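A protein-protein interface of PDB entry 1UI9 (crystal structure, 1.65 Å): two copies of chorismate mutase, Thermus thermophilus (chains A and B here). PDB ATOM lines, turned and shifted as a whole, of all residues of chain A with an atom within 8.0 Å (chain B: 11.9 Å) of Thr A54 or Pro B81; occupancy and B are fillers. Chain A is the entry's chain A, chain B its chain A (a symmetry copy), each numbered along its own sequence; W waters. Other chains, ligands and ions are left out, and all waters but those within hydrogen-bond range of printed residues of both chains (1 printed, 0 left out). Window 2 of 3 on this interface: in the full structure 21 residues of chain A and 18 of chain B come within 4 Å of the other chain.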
ATOM      1  N   GLU A  13      -8.268   2.014  26.011  1.00  0.00           N
ATOM      2  CA  GLU A  13      -8.997   1.339  24.948  1.00  0.00           C
ATOM      3  C   GLU A  13      -8.156   0.258  24.298  1.00  0.00           C
ATOM      4  O   GLU A  13      -6.929   0.361  24.229  1.00  0.00           O
ATOM      5  CB  GLU A  13      -9.418   2.331  23.865  1.00  0.00           C
ATOM      6  CG  GLU A  13     -10.199   3.527  24.357  1.00  0.00           C
ATOM      7  CD  GLU A  13     -10.735   4.356  23.208  1.00  0.00           C
ATOM      8  OE1 GLU A  13      -9.938   4.722  22.316  1.00  0.00           O
ATOM      9  OE2 GLU A  13     -11.952   4.636  23.196  1.00  0.00           O
ATOM     10  N   ASP A  14      -8.829  -0.773  23.803  1.00  0.00           N
ATOM     11  CA  ASP A  14      -8.150  -1.872  23.137  1.00  0.00           C
ATOM     12  C   ASP A  14      -7.962  -1.597  21.641  1.00  0.00           C
ATOM     13  O   ASP A  14      -8.754  -2.045  20.805  1.00  0.00           O
ATOM     14  CB  ASP A  14      -8.932  -3.174  23.353  1.00  0.00           C
ATOM     15  CG  ASP A  14      -8.331  -4.350  22.601  1.00  0.00           C
ATOM     16  OD1 ASP A  14      -7.116  -4.319  22.302  1.00  0.00           O
ATOM     17  OD2 ASP A  14      -9.077  -5.313  22.314  1.00  0.00           O
ATOM     18  N   THR A  15      -6.921  -0.831  21.322  1.00  0.00           N
ATOM     19  CA  THR A  15      -6.572  -0.502  19.940  1.00  0.00           C
ATOM     20  C   THR A  15      -5.055  -0.599  19.805  1.00  0.00           C
ATOM     21  O   THR A  15      -4.325  -0.380  20.776  1.00  0.00           O
ATOM     22  CB  THR A  15      -6.986   0.936  19.550  1.00  0.00           C
ATOM     23  OG1 THR A  15      -6.231   1.879  20.323  1.00  0.00           O
ATOM     24  CG2 THR A  15      -8.468   1.154  19.786  1.00  0.00           C
ATOM     25  N   PRO A  16      -4.555  -0.921  18.602  1.00  0.00           N
ATOM     26  CA  PRO A  16      -3.105  -1.028  18.414  1.00  0.00           C
ATOM     27  C   PRO A  16      -2.408   0.294  18.734  1.00  0.00           C
ATOM     28  O   PRO A  16      -1.324   0.314  19.312  1.00  0.00           O
ATOM     29  CB  PRO A  16      -2.968  -1.405  16.939  1.00  0.00           C
ATOM     30  CG  PRO A  16      -4.256  -2.086  16.630  1.00  0.00           C
ATOM     31  CD  PRO A  16      -5.277  -1.274  17.366  1.00  0.00           C
ATOM     32  N   ILE A  19      -2.144   0.882  22.529  1.00  0.00           N
ATOM     33  CA  ILE A  19      -1.160  -0.056  23.066  1.00  0.00           C
ATOM     34  C   ILE A  19       0.266   0.375  22.696  1.00  0.00           C
ATOM     35  O   ILE A  19       1.188   0.291  23.510  1.00  0.00           O
ATOM     36  CB  ILE A  19      -1.433  -1.488  22.532  1.00  0.00           C
ATOM     37  CG1 ILE A  19      -2.785  -1.983  23.045  1.00  0.00           C
ATOM     38  CG2 ILE A  19      -0.317  -2.435  22.963  1.00  0.00           C
ATOM     39  CD1 ILE A  19      -3.269  -3.271  22.377  1.00  0.00           C
ATOM     40  N   VAL A  49       1.154  -9.363  28.053  1.00  0.00           N
ATOM     41  CA  VAL A  49      -0.027  -8.616  27.636  1.00  0.00           C
ATOM     42  C   VAL A  49      -1.252  -9.331  28.185  1.00  0.00           C
ATOM     43  O   VAL A  49      -1.341 -10.553  28.111  1.00  0.00           O
ATOM     44  CB  VAL A  49      -0.117  -8.575  26.085  1.00  0.00           C
ATOM     45  CG1 VAL A  49      -1.348  -7.791  25.642  1.00  0.00           C
ATOM     46  CG2 VAL A  49       1.162  -7.964  25.502  1.00  0.00           C
ATOM     47  N   THR A  50      -2.195  -8.584  28.743  1.00  0.00           N
ATOM     48  CA  THR A  50      -3.400  -9.207  29.280  1.00  0.00           C
ATOM     49  C   THR A  50      -4.331  -9.623  28.141  1.00  0.00           C
ATOM     50  O   THR A  50      -4.285  -9.055  27.048  1.00  0.00           O
ATOM     51  CB  THR A  50      -4.130  -8.261  30.248  1.00  0.00           C
ATOM     52  OG1 THR A  50      -4.318  -6.991  29.619  1.00  0.00           O
ATOM     53  CG2 THR A  50      -3.313  -8.073  31.528  1.00  0.00           C
ATOM     54  N   GLU A  51      -5.179 -10.610  28.406  1.00  0.00           N
ATOM     55  CA  GLU A  51      -6.082 -11.145  27.386  1.00  0.00           C
ATOM     56  C   GLU A  51      -7.146 -10.197  26.838  1.00  0.00           C
ATOM     57  O   GLU A  51      -7.759 -10.493  25.810  1.00  0.00           O
ATOM     58  CB  GLU A  51      -6.759 -12.417  27.899  1.00  0.00           C
ATOM     59  CG  GLU A  51      -7.481 -12.242  29.211  1.00  0.00           C
ATOM     60  CD  GLU A  51      -8.397 -13.403  29.516  1.00  0.00           C
ATOM     61  OE1 GLU A  51      -8.166 -14.506  28.975  1.00  0.00           O
ATOM     62  OE2 GLU A  51      -9.342 -13.213  30.307  1.00  0.00           O
ATOM     63  N   ASP A  52      -7.370  -9.072  27.509  1.00  0.00           N
ATOM     64  CA  ASP A  52      -8.351  -8.097  27.040  1.00  0.00           C
ATOM     65  C   ASP A  52      -7.759  -7.093  26.048  1.00  0.00           C
ATOM     66  O   ASP A  52      -8.408  -6.114  25.687  1.00  0.00           O
ATOM     67  CB  ASP A  52      -9.000  -7.362  28.215  1.00  0.00           C
ATOM     68  CG  ASP A  52      -7.996  -6.844  29.218  1.00  0.00           C
ATOM     69  OD1 ASP A  52      -6.800  -6.735  28.879  1.00  0.00           O
ATOM     70  OD2 ASP A  52      -8.421  -6.529  30.350  1.00  0.00           O
ATOM     71  N   LEU A  53      -6.520  -7.327  25.629  1.00  0.00           N
ATOM     72  CA  LEU A  53      -5.880  -6.479  24.623  1.00  0.00           C
ATOM     73  C   LEU A  53      -5.719  -7.415  23.429  1.00  0.00           C
ATOM     74  O   LEU A  53      -5.270  -8.553  23.575  1.00  0.00           O
ATOM     75  CB  LEU A  53      -4.531  -5.942  25.114  1.00  0.00           C
ATOM     76  CG  LEU A  53      -4.662  -4.905  26.241  1.00  0.00           C
ATOM     77  CD1 LEU A  53      -3.278  -4.512  26.743  1.00  0.00           C
ATOM     78  CD2 LEU A  53      -5.420  -3.686  25.734  1.00  0.00           C
ATOM     79  N   THR A  54      -6.084  -6.942  22.246  1.00  0.00           N
ATOM     80  CA  THR A  54      -6.053  -7.800  21.073  1.00  0.00           C
ATOM     81  C   THR A  54      -4.885  -7.617  20.116  1.00  0.00           C
ATOM     82  O   THR A  54      -3.991  -8.466  20.043  1.00  0.00           O
ATOM     83  CB  THR A  54      -7.381  -7.657  20.305  1.00  0.00           C
ATOM     84  OG1 THR A  54      -8.471  -7.763  21.232  1.00  0.00           O
ATOM     85  CG2 THR A  54      -7.522  -8.757  19.265  1.00  0.00           C
ATOM     86  N   PHE A  55      -4.896  -6.521  19.367  1.00  0.00           N
ATOM     87  CA  PHE A  55      -3.825  -6.256  18.420  1.00  0.00           C
ATOM     88  C   PHE A  55      -2.716  -5.484  19.128  1.00  0.00           C
ATOM     89  O   PHE A  55      -2.552  -4.274  18.948  1.00  0.00           O
ATOM     90  CB  PHE A  55      -4.395  -5.484  17.223  1.00  0.00           C
ATOM     91  CG  PHE A  55      -5.393  -6.282  16.425  1.00  0.00           C
ATOM     92  CD1 PHE A  55      -4.961  -7.276  15.548  1.00  0.00           C
ATOM     93  CD2 PHE A  55      -6.761  -6.095  16.602  1.00  0.00           C
ATOM     94  CE1 PHE A  55      -5.877  -8.079  14.866  1.00  0.00           C
ATOM     95  CE2 PHE A  55      -7.686  -6.891  15.926  1.00  0.00           C
ATOM     96  CZ  PHE A  55      -7.241  -7.887  15.055  1.00  0.00           C
ATOM     97  N   ALA A  56      -1.963  -6.213  19.948  1.00  0.00           N
ATOM     98  CA  ALA A  56      -0.873  -5.643  20.732  1.00  0.00           C
ATOM     99  C   ALA A  56       0.481  -5.951  20.110  1.00  0.00           C
ATOM    100  O   ALA A  56       0.889  -7.111  20.016  1.00  0.00           O
ATOM    101  CB  ALA A  56      -0.934  -6.184  22.163  1.00  0.00           C
ATOM    102  N   PHE A  57       1.182  -4.899  19.700  1.00  0.00           N
ATOM    103  CA  PHE A  57       2.489  -5.032  19.069  1.00  0.00           C
ATOM    104  C   PHE A  57       3.518  -4.231  19.862  1.00  0.00           C
ATOM    105  O   PHE A  57       4.141  -3.307  19.330  1.00  0.00           O
ATOM    106  CB  PHE A  57       2.430  -4.494  17.635  1.00  0.00           C
ATOM    107  CG  PHE A  57       1.328  -5.091  16.804  1.00  0.00           C
ATOM    108  CD1 PHE A  57       1.403  -6.412  16.366  1.00  0.00           C
ATOM    109  CD2 PHE A  57       0.215  -4.332  16.459  1.00  0.00           C
ATOM    110  CE1 PHE A  57       0.383  -6.969  15.593  1.00  0.00           C
ATOM    111  CE2 PHE A  57      -0.813  -4.880  15.684  1.00  0.00           C
ATOM    112  CZ  PHE A  57      -0.727  -6.202  15.252  1.00  0.00           C
ATOM    113  N   PRO A  58       3.723  -4.584  21.141  1.00  0.00           N
ATOM    114  CA  PRO A  58       4.695  -3.851  21.961  1.00  0.00           C
ATOM    115  C   PRO A  58       6.088  -3.781  21.342  1.00  0.00           C
ATOM    116  O   PRO A  58       6.814  -2.804  21.532  1.00  0.00           O
ATOM    117  CB  PRO A  58       4.671  -4.607  23.286  1.00  0.00           C
ATOM    118  CG  PRO A  58       4.332  -6.021  22.863  1.00  0.00           C
ATOM    119  CD  PRO A  58       3.239  -5.787  21.845  1.00  0.00           C
ATOM    120  N   ARG A  76       1.568 -14.137  26.986  1.00  0.00           N
ATOM    121  CA  ARG A  76       0.288 -13.833  27.590  1.00  0.00           C
ATOM    122  C   ARG A  76       0.411 -13.826  29.118  1.00  0.00           C
ATOM    123  O   ARG A  76       0.920 -14.775  29.717  1.00  0.00           O
ATOM    124  CB  ARG A  76      -0.764 -14.865  27.159  1.00  0.00           C
ATOM    125  CG  ARG A  76      -1.990 -14.898  28.064  1.00  0.00           C
ATOM    126  CD  ARG A  76      -3.248 -15.301  27.316  1.00  0.00           C
ATOM    127  NE  ARG A  76      -3.686 -14.254  26.398  1.00  0.00           N
ATOM    128  CZ  ARG A  76      -4.746 -14.357  25.605  1.00  0.00           C
ATOM    129  NH1 ARG A  76      -5.482 -15.462  25.621  1.00  0.00           N
ATOM    130  NH2 ARG A  76      -5.059 -13.366  24.781  1.00  0.00           N
ATOM    131  N   ARG A  86      -6.507  -4.459  30.820  1.00  0.00           N
ATOM    132  CA  ARG A  86      -5.685  -3.812  29.804  1.00  0.00           C
ATOM    133  C   ARG A  86      -4.315  -3.346  30.278  1.00  0.00           C
ATOM    134  O   ARG A  86      -4.006  -2.152  30.259  1.00  0.00           O
ATOM    135  CB  ARG A  86      -6.468  -2.635  29.210  1.00  0.00           C
ATOM    136  CG  ARG A  86      -7.793  -3.057  28.589  1.00  0.00           C
ATOM    137  CD  ARG A  86      -8.497  -1.876  27.920  1.00  0.00           C
ATOM    138  NE  ARG A  86      -8.767  -0.807  28.875  1.00  0.00           N
ATOM    139  CZ  ARG A  86      -9.714  -0.850  29.808  1.00  0.00           C
ATOM    140  NH1 ARG A  86     -10.505  -1.909  29.920  1.00  0.00           N
ATOM    141  NH2 ARG A  86      -9.857   0.166  30.647  1.00  0.00           N
ATOM    142  N   THR B  50       2.761 -20.397  19.639  1.00  0.00           N
ATOM    143  CA  THR B  50       1.504 -19.765  19.248  1.00  0.00           C
ATOM    144  C   THR B  50       0.331 -20.699  19.544  1.00  0.00           C
ATOM    145  O   THR B  50       0.493 -21.920  19.599  1.00  0.00           O
ATOM    146  CB  THR B  50       1.516 -19.377  17.761  1.00  0.00           C
ATOM    147  OG1 THR B  50       1.909 -20.507  16.978  1.00  0.00           O
ATOM    148  CG2 THR B  50       2.499 -18.229  17.517  1.00  0.00           C
ATOM    149  N   GLU B  51      -0.851 -20.119  19.725  1.00  0.00           N
ATOM    150  CA  GLU B  51      -2.043 -20.892  20.074  1.00  0.00           C
ATOM    151  C   GLU B  51      -2.544 -21.898  19.039  1.00  0.00           C
ATOM    152  O   GLU B  51      -3.370 -22.753  19.366  1.00  0.00           O
ATOM    153  CB  GLU B  51      -3.187 -19.951  20.453  1.00  0.00           C
ATOM    154  CG  GLU B  51      -3.509 -18.921  19.400  1.00  0.00           C
ATOM    155  CD  GLU B  51      -4.830 -18.237  19.658  1.00  0.00           C
ATOM    156  OE1 GLU B  51      -5.281 -18.223  20.824  1.00  0.00           O
ATOM    157  OE2 GLU B  51      -5.413 -17.703  18.694  1.00  0.00           O
ATOM    158  N   ASP B  52      -2.057 -21.803  17.806  1.00  0.00           N
ATOM    159  CA  ASP B  52      -2.461 -22.740  16.762  1.00  0.00           C
ATOM    160  C   ASP B  52      -1.599 -24.005  16.737  1.00  0.00           C
ATOM    161  O   ASP B  52      -1.703 -24.815  15.818  1.00  0.00           O
ATOM    162  CB  ASP B  52      -2.456 -22.068  15.387  1.00  0.00           C
ATOM    163  CG  ASP B  52      -1.190 -21.293  15.110  1.00  0.00           C
ATOM    164  OD1 ASP B  52      -0.173 -21.525  15.796  1.00  0.00           O
ATOM    165  OD2 ASP B  52      -1.216 -20.455  14.184  1.00  0.00           O
ATOM    166  N   ARG B  76       2.844 -19.207  26.470  1.00  0.00           N
ATOM    167  CA  ARG B  76       2.008 -18.922  25.322  1.00  0.00           C
ATOM    168  C   ARG B  76       2.348 -17.543  24.748  1.00  0.00           C
ATOM    169  O   ARG B  76       2.386 -16.546  25.471  1.00  0.00           O
ATOM    170  CB  ARG B  76       0.525 -18.969  25.719  1.00  0.00           C
ATOM    171  CG  ARG B  76      -0.392 -18.263  24.726  1.00  0.00           C
ATOM    172  CD  ARG B  76      -1.776 -18.884  24.678  1.00  0.00           C
ATOM    173  NE  ARG B  76      -1.752 -20.202  24.051  1.00  0.00           N
ATOM    174  CZ  ARG B  76      -2.823 -20.973  23.902  1.00  0.00           C
ATOM    175  NH1 ARG B  76      -4.007 -20.555  24.333  1.00  0.00           N
ATOM    176  NH2 ARG B  76      -2.708 -22.170  23.343  1.00  0.00           N
ATOM    177  N   GLU B  77       2.620 -17.500  23.447  1.00  0.00           N
ATOM    178  CA  GLU B  77       2.916 -16.246  22.745  1.00  0.00           C
ATOM    179  C   GLU B  77       1.618 -15.439  22.700  1.00  0.00           C
ATOM    180  O   GLU B  77       0.547 -16.016  22.522  1.00  0.00           O
ATOM    181  CB  GLU B  77       3.376 -16.575  21.318  1.00  0.00           C
ATOM    182  CG  GLU B  77       3.462 -15.400  20.336  1.00  0.00           C
ATOM    183  CD  GLU B  77       4.615 -14.456  20.619  1.00  0.00           C
ATOM    184  OE1 GLU B  77       5.645 -14.901  21.156  1.00  0.00           O
ATOM    185  OE2 GLU B  77       4.502 -13.259  20.278  1.00  0.00           O
ATOM    186  N   VAL B  78       1.695 -14.120  22.871  1.00  0.00           N
ATOM    187  CA  VAL B  78       0.481 -13.298  22.816  1.00  0.00           C
ATOM    188  C   VAL B  78      -0.251 -13.636  21.509  1.00  0.00           C
ATOM    189  O   VAL B  78       0.290 -13.436  20.423  1.00  0.00           O
ATOM    190  CB  VAL B  78       0.827 -11.791  22.852  1.00  0.00           C
ATOM    191  CG1 VAL B  78      -0.448 -10.967  22.736  1.00  0.00           C
ATOM    192  CG2 VAL B  78       1.557 -11.448  24.158  1.00  0.00           C
ATOM    193  N   PRO B  79      -1.497 -14.145  21.597  1.00  0.00           N
ATOM    194  CA  PRO B  79      -2.293 -14.528  20.420  1.00  0.00           C
ATOM    195  C   PRO B  79      -2.953 -13.442  19.580  1.00  0.00           C
ATOM    196  O   PRO B  79      -4.180 -13.328  19.547  1.00  0.00           O
ATOM    197  CB  PRO B  79      -3.321 -15.480  21.009  1.00  0.00           C
ATOM    198  CG  PRO B  79      -3.611 -14.833  22.323  1.00  0.00           C
ATOM    199  CD  PRO B  79      -2.222 -14.480  22.838  1.00  0.00           C
ATOM    200  N   VAL B  80      -2.145 -12.672  18.871  1.00  0.00           N
ATOM    201  CA  VAL B  80      -2.668 -11.602  18.034  1.00  0.00           C
ATOM    202  C   VAL B  80      -3.374 -12.195  16.813  1.00  0.00           C
ATOM    203  O   VAL B  80      -2.778 -12.972  16.063  1.00  0.00           O
ATOM    204  CB  VAL B  80      -1.527 -10.692  17.566  1.00  0.00           C
ATOM    205  CG1 VAL B  80      -2.074  -9.580  16.685  1.00  0.00           C
ATOM    206  CG2 VAL B  80      -0.801 -10.123  18.776  1.00  0.00           C
ATOM    207  N   PRO B  81      -4.655 -11.844  16.601  1.00  0.00           N
ATOM    208  CA  PRO B  81      -5.388 -12.375  15.449  1.00  0.00           C
ATOM    209  C   PRO B  81      -4.681 -12.038  14.141  1.00  0.00           C
ATOM    210  O   PRO B  81      -4.154 -10.936  13.983  1.00  0.00           O
ATOM    211  CB  PRO B  81      -6.745 -11.683  15.549  1.00  0.00           C
ATOM    212  CG  PRO B  81      -6.906 -11.449  17.020  1.00  0.00           C
ATOM    213  CD  PRO B  81      -5.525 -10.981  17.420  1.00  0.00           C
ATOM    214  N   GLY B  82      -4.665 -12.990  13.215  1.00  0.00           N
ATOM    215  CA  GLY B  82      -4.041 -12.764  11.922  1.00  0.00           C
ATOM    216  C   GLY B  82      -2.525 -12.718  11.877  1.00  0.00           C
ATOM    217  O   GLY B  82      -1.950 -12.485  10.815  1.00  0.00           O
ATOM    218  N   SER B  83      -1.866 -12.935  13.010  1.00  0.00           N
ATOM    219  CA  SER B  83      -0.407 -12.913  13.031  1.00  0.00           C
ATOM    220  C   SER B  83       0.132 -14.191  12.380  1.00  0.00           C
ATOM    221  O   SER B  83      -0.623 -15.136  12.136  1.00  0.00           O
ATOM    222  CB  SER B  83       0.101 -12.788  14.472  1.00  0.00           C
ATOM    223  OG  SER B  83      -0.413 -13.820  15.288  1.00  0.00           O
ATOM    224  N   LEU B  84       1.429 -14.211  12.086  1.00  0.00           N
ATOM    225  CA  LEU B  84       2.060 -15.366  11.459  1.00  0.00           C
ATOM    226  C   LEU B  84       1.688 -16.638  12.222  1.00  0.00           C
ATOM    227  O   LEU B  84       1.928 -16.751  13.421  1.00  0.00           O
ATOM    228  CB  LEU B  84       3.582 -15.188  11.435  1.00  0.00           C
ATOM    229  CG  LEU B  84       4.387 -16.242  10.671  1.00  0.00           C
ATOM    230  CD1 LEU B  84       4.051 -16.167   9.185  1.00  0.00           C
ATOM    231  CD2 LEU B  84       5.872 -16.006  10.891  1.00  0.00           C
ATOM    232  N   PRO B  85       1.096 -17.614  11.528  1.00  0.00           N
ATOM    233  CA  PRO B  85       0.700 -18.859  12.192  1.00  0.00           C
ATOM    234  C   PRO B  85       1.785 -19.907  12.441  1.00  0.00           C
ATOM    235  O   PRO B  85       2.813 -19.951  11.758  1.00  0.00           O
ATOM    236  CB  PRO B  85      -0.408 -19.384  11.283  1.00  0.00           C
ATOM    237  CG  PRO B  85       0.059 -18.964   9.927  1.00  0.00           C
ATOM    238  CD  PRO B  85       0.577 -17.555  10.149  1.00  0.00           C
ATOM    239  N   ARG B  86       1.532 -20.737  13.450  1.00  0.00           N
ATOM    240  CA  ARG B  86       2.403 -21.846  13.821  1.00  0.00           C
ATOM    241  C   ARG B  86       3.873 -21.487  13.995  1.00  0.00           C
ATOM    242  O   ARG B  86       4.740 -21.989  13.275  1.00  0.00           O
ATOM    243  CB  ARG B  86       2.251 -22.964  12.782  1.00  0.00           C
ATOM    244  CG  ARG B  86       0.820 -23.469  12.660  1.00  0.00           C
ATOM    245  CD  ARG B  86       0.724 -24.648  11.691  1.00  0.00           C
ATOM    246  NE  ARG B  86       1.186 -24.279  10.357  1.00  0.00           N
ATOM    247  CZ  ARG B  86       0.505 -23.517   9.506  1.00  0.00           C
ATOM    248  NH1 ARG B  86      -0.688 -23.038   9.834  1.00  0.00           N
ATOM    249  NH2 ARG B  86       1.030 -23.217   8.327  1.00  0.00           N
ATOM    250  N   VAL B  87       4.153 -20.644  14.980  1.00  0.00           N
ATOM    251  CA  VAL B  87       5.518 -20.210  15.233  1.00  0.00           C
ATOM    252  C   VAL B  87       6.054 -20.639  16.591  1.00  0.00           C
ATOM    253  O   VAL B  87       5.354 -20.581  17.607  1.00  0.00           O
ATOM    254  CB  VAL B  87       5.636 -18.661  15.146  1.00  0.00           C
ATOM    255  CG1 VAL B  87       7.096 -18.237  15.218  1.00  0.00           C
ATOM    256  CG2 VAL B  87       5.002 -18.155  13.858  1.00  0.00           C
ATOM    257  N   ARG B  89       9.070 -19.669  19.020  1.00  0.00           N
ATOM    258  CA  ARG B  89      10.078 -18.631  19.223  1.00  0.00           C
ATOM    259  C   ARG B  89      10.984 -18.997  20.383  1.00  0.00           C
ATOM    260  O   ARG B  89      10.569 -19.672  21.322  1.00  0.00           O
ATOM    261  CB  ARG B  89       9.418 -17.283  19.501  1.00  0.00           C
ATOM    262  CG  ARG B  89       8.713 -16.663  18.294  1.00  0.00           C
ATOM    263  CD  ARG B  89       8.088 -15.328  18.676  1.00  0.00           C
ATOM    264  NE  ARG B  89       7.537 -14.578  17.545  1.00  0.00           N
ATOM    265  CZ  ARG B  89       6.345 -14.793  16.988  1.00  0.00           C
ATOM    266  NH1 ARG B  89       5.547 -15.749  17.441  1.00  0.00           N
ATOM    267  NH2 ARG B  89       5.933 -14.026  15.987  1.00  0.00           N
ATOM    268  N   ARG B 113       9.664 -13.649   7.547  1.00  0.00           N
ATOM    269  CA  ARG B 113       8.737 -12.546   7.313  1.00  0.00           C
ATOM    270  C   ARG B 113       8.556 -11.680   8.558  1.00  0.00           C
ATOM    271  O   ARG B 113       8.057 -10.556   8.477  1.00  0.00           O
ATOM    272  CB  ARG B 113       7.375 -13.095   6.877  1.00  0.00           C
ATOM    273  CG  ARG B 113       7.429 -13.988   5.643  1.00  0.00           C
ATOM    274  CD  ARG B 113       6.111 -14.721   5.432  1.00  0.00           C
ATOM    275  NE  ARG B 113       4.999 -13.809   5.175  1.00  0.00           N
ATOM    276  CZ  ARG B 113       3.720 -14.174   5.173  1.00  0.00           C
ATOM    277  NH1 ARG B 113       3.386 -15.434   5.420  1.00  0.00           N
ATOM    278  NH2 ARG B 113       2.772 -13.281   4.923  1.00  0.00           N
ATOM    279  N   LEU B 114       8.959 -12.208   9.710  1.00  0.00           N
ATOM    280  CA  LEU B 114       8.826 -11.479  10.966  1.00  0.00           C
ATOM    281  C   LEU B 114       9.780 -10.291  11.053  1.00  0.00           C
ATOM    282  O   LEU B 114       9.466  -9.286  11.690  1.00  0.00           O
ATOM    283  CB  LEU B 114       9.060 -12.424  12.152  1.00  0.00           C
ATOM    284  CG  LEU B 114       8.063 -13.581  12.286  1.00  0.00           C
ATOM    285  CD1 LEU B 114       8.494 -14.503  13.421  1.00  0.00           C
ATOM    286  CD2 LEU B 114       6.665 -13.034  12.542  1.00  0.00           C
HETATM  287  O   HOH W   1      -4.009 -11.095  21.297  1.00  0.00           O
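N of Arg A76 lies within hydrogen-bond range of O of Arg B76 (3.0 Å).
The side-chain carboxylate of Asp A14 sits at hydrogen-bond distance from the side-chain hydroxyl of Thr A54 (2.7 Å). O of Val B80 is in hydrogen-bond range of OG of Ser B83 (2.6 Å).
Among the printed residues, merely in contact across the chains: Val A49 with Val B78 (3.8 Å), Thr A54 with Val B80 (3.8 Å), Thr A54 with Pro B81 (3.5 Å), Phe A55 with Val B80 (3.9 Å), Phe A55 with Pro B81 (3.5 Å), Ala A56 with Val B80 (3.7 Å), Phe A57 with Val B80 (3.7 Å), Arg A76 with Val B78 (3.9 Å) and Arg A76 with Pro B79 (3.2 Å).
Of chain B, only Val B80 and Pro B81 come within 4 Å of Thr A54. Of chain A, only Thr A54 and Phe A55 come within 4 Å of Pro B81. No residue of chain B comes within 4 Å of Asp A14. Of chain B, only Val B80 and Pro B81 come within 4 Å of Phe A55. Of chain B, only Val B80 comes within 4 Å of Ala A56. Of chain A, only Thr A54, Phe A55, Ala A56 and Phe A57 come within 4 Å of Val B80. Of the printed residues of chain B, Phe A57 touches Val B80 (3.7 Å). Of the printed residues of chain A, Arg B76 touches Arg A76. Of the printed residues of chain B, Arg A76 touches Arg B76 (3.0 Å), Val B78 (3.9 Å) and Pro B79 (3.2 Å). Of the printed residues of chain A, Pro B79 touches Arg A76 (3.2 Å). Thr B50 touches none of the printed residues of chain A. The nearest printed residue of chain A that does not touch Val B78 is Ala A56 (4.8 Å).
Of the 18 printed residues of chain B, 5 touch a printed residue of chain A. Hydrophobic or aromatic side chains of chain A that line the printed part of chain B: Val A49, Phe A55 and Phe A57.
Arg B76 touches its own counterpart, Arg A76. Positions printed for both chains: 50, 51, 52, 76 and 86. Of the 10 pairs that touch across the chains among the printed residues, 1 has its exchanged pair printed and touching as well.
Water W1 lies within hydrogen-bond range of the backbone carbonyl oxygen of Pro B79, the backbone carbonyl oxygen of Thr A54 and the backbone NH of Val B80.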
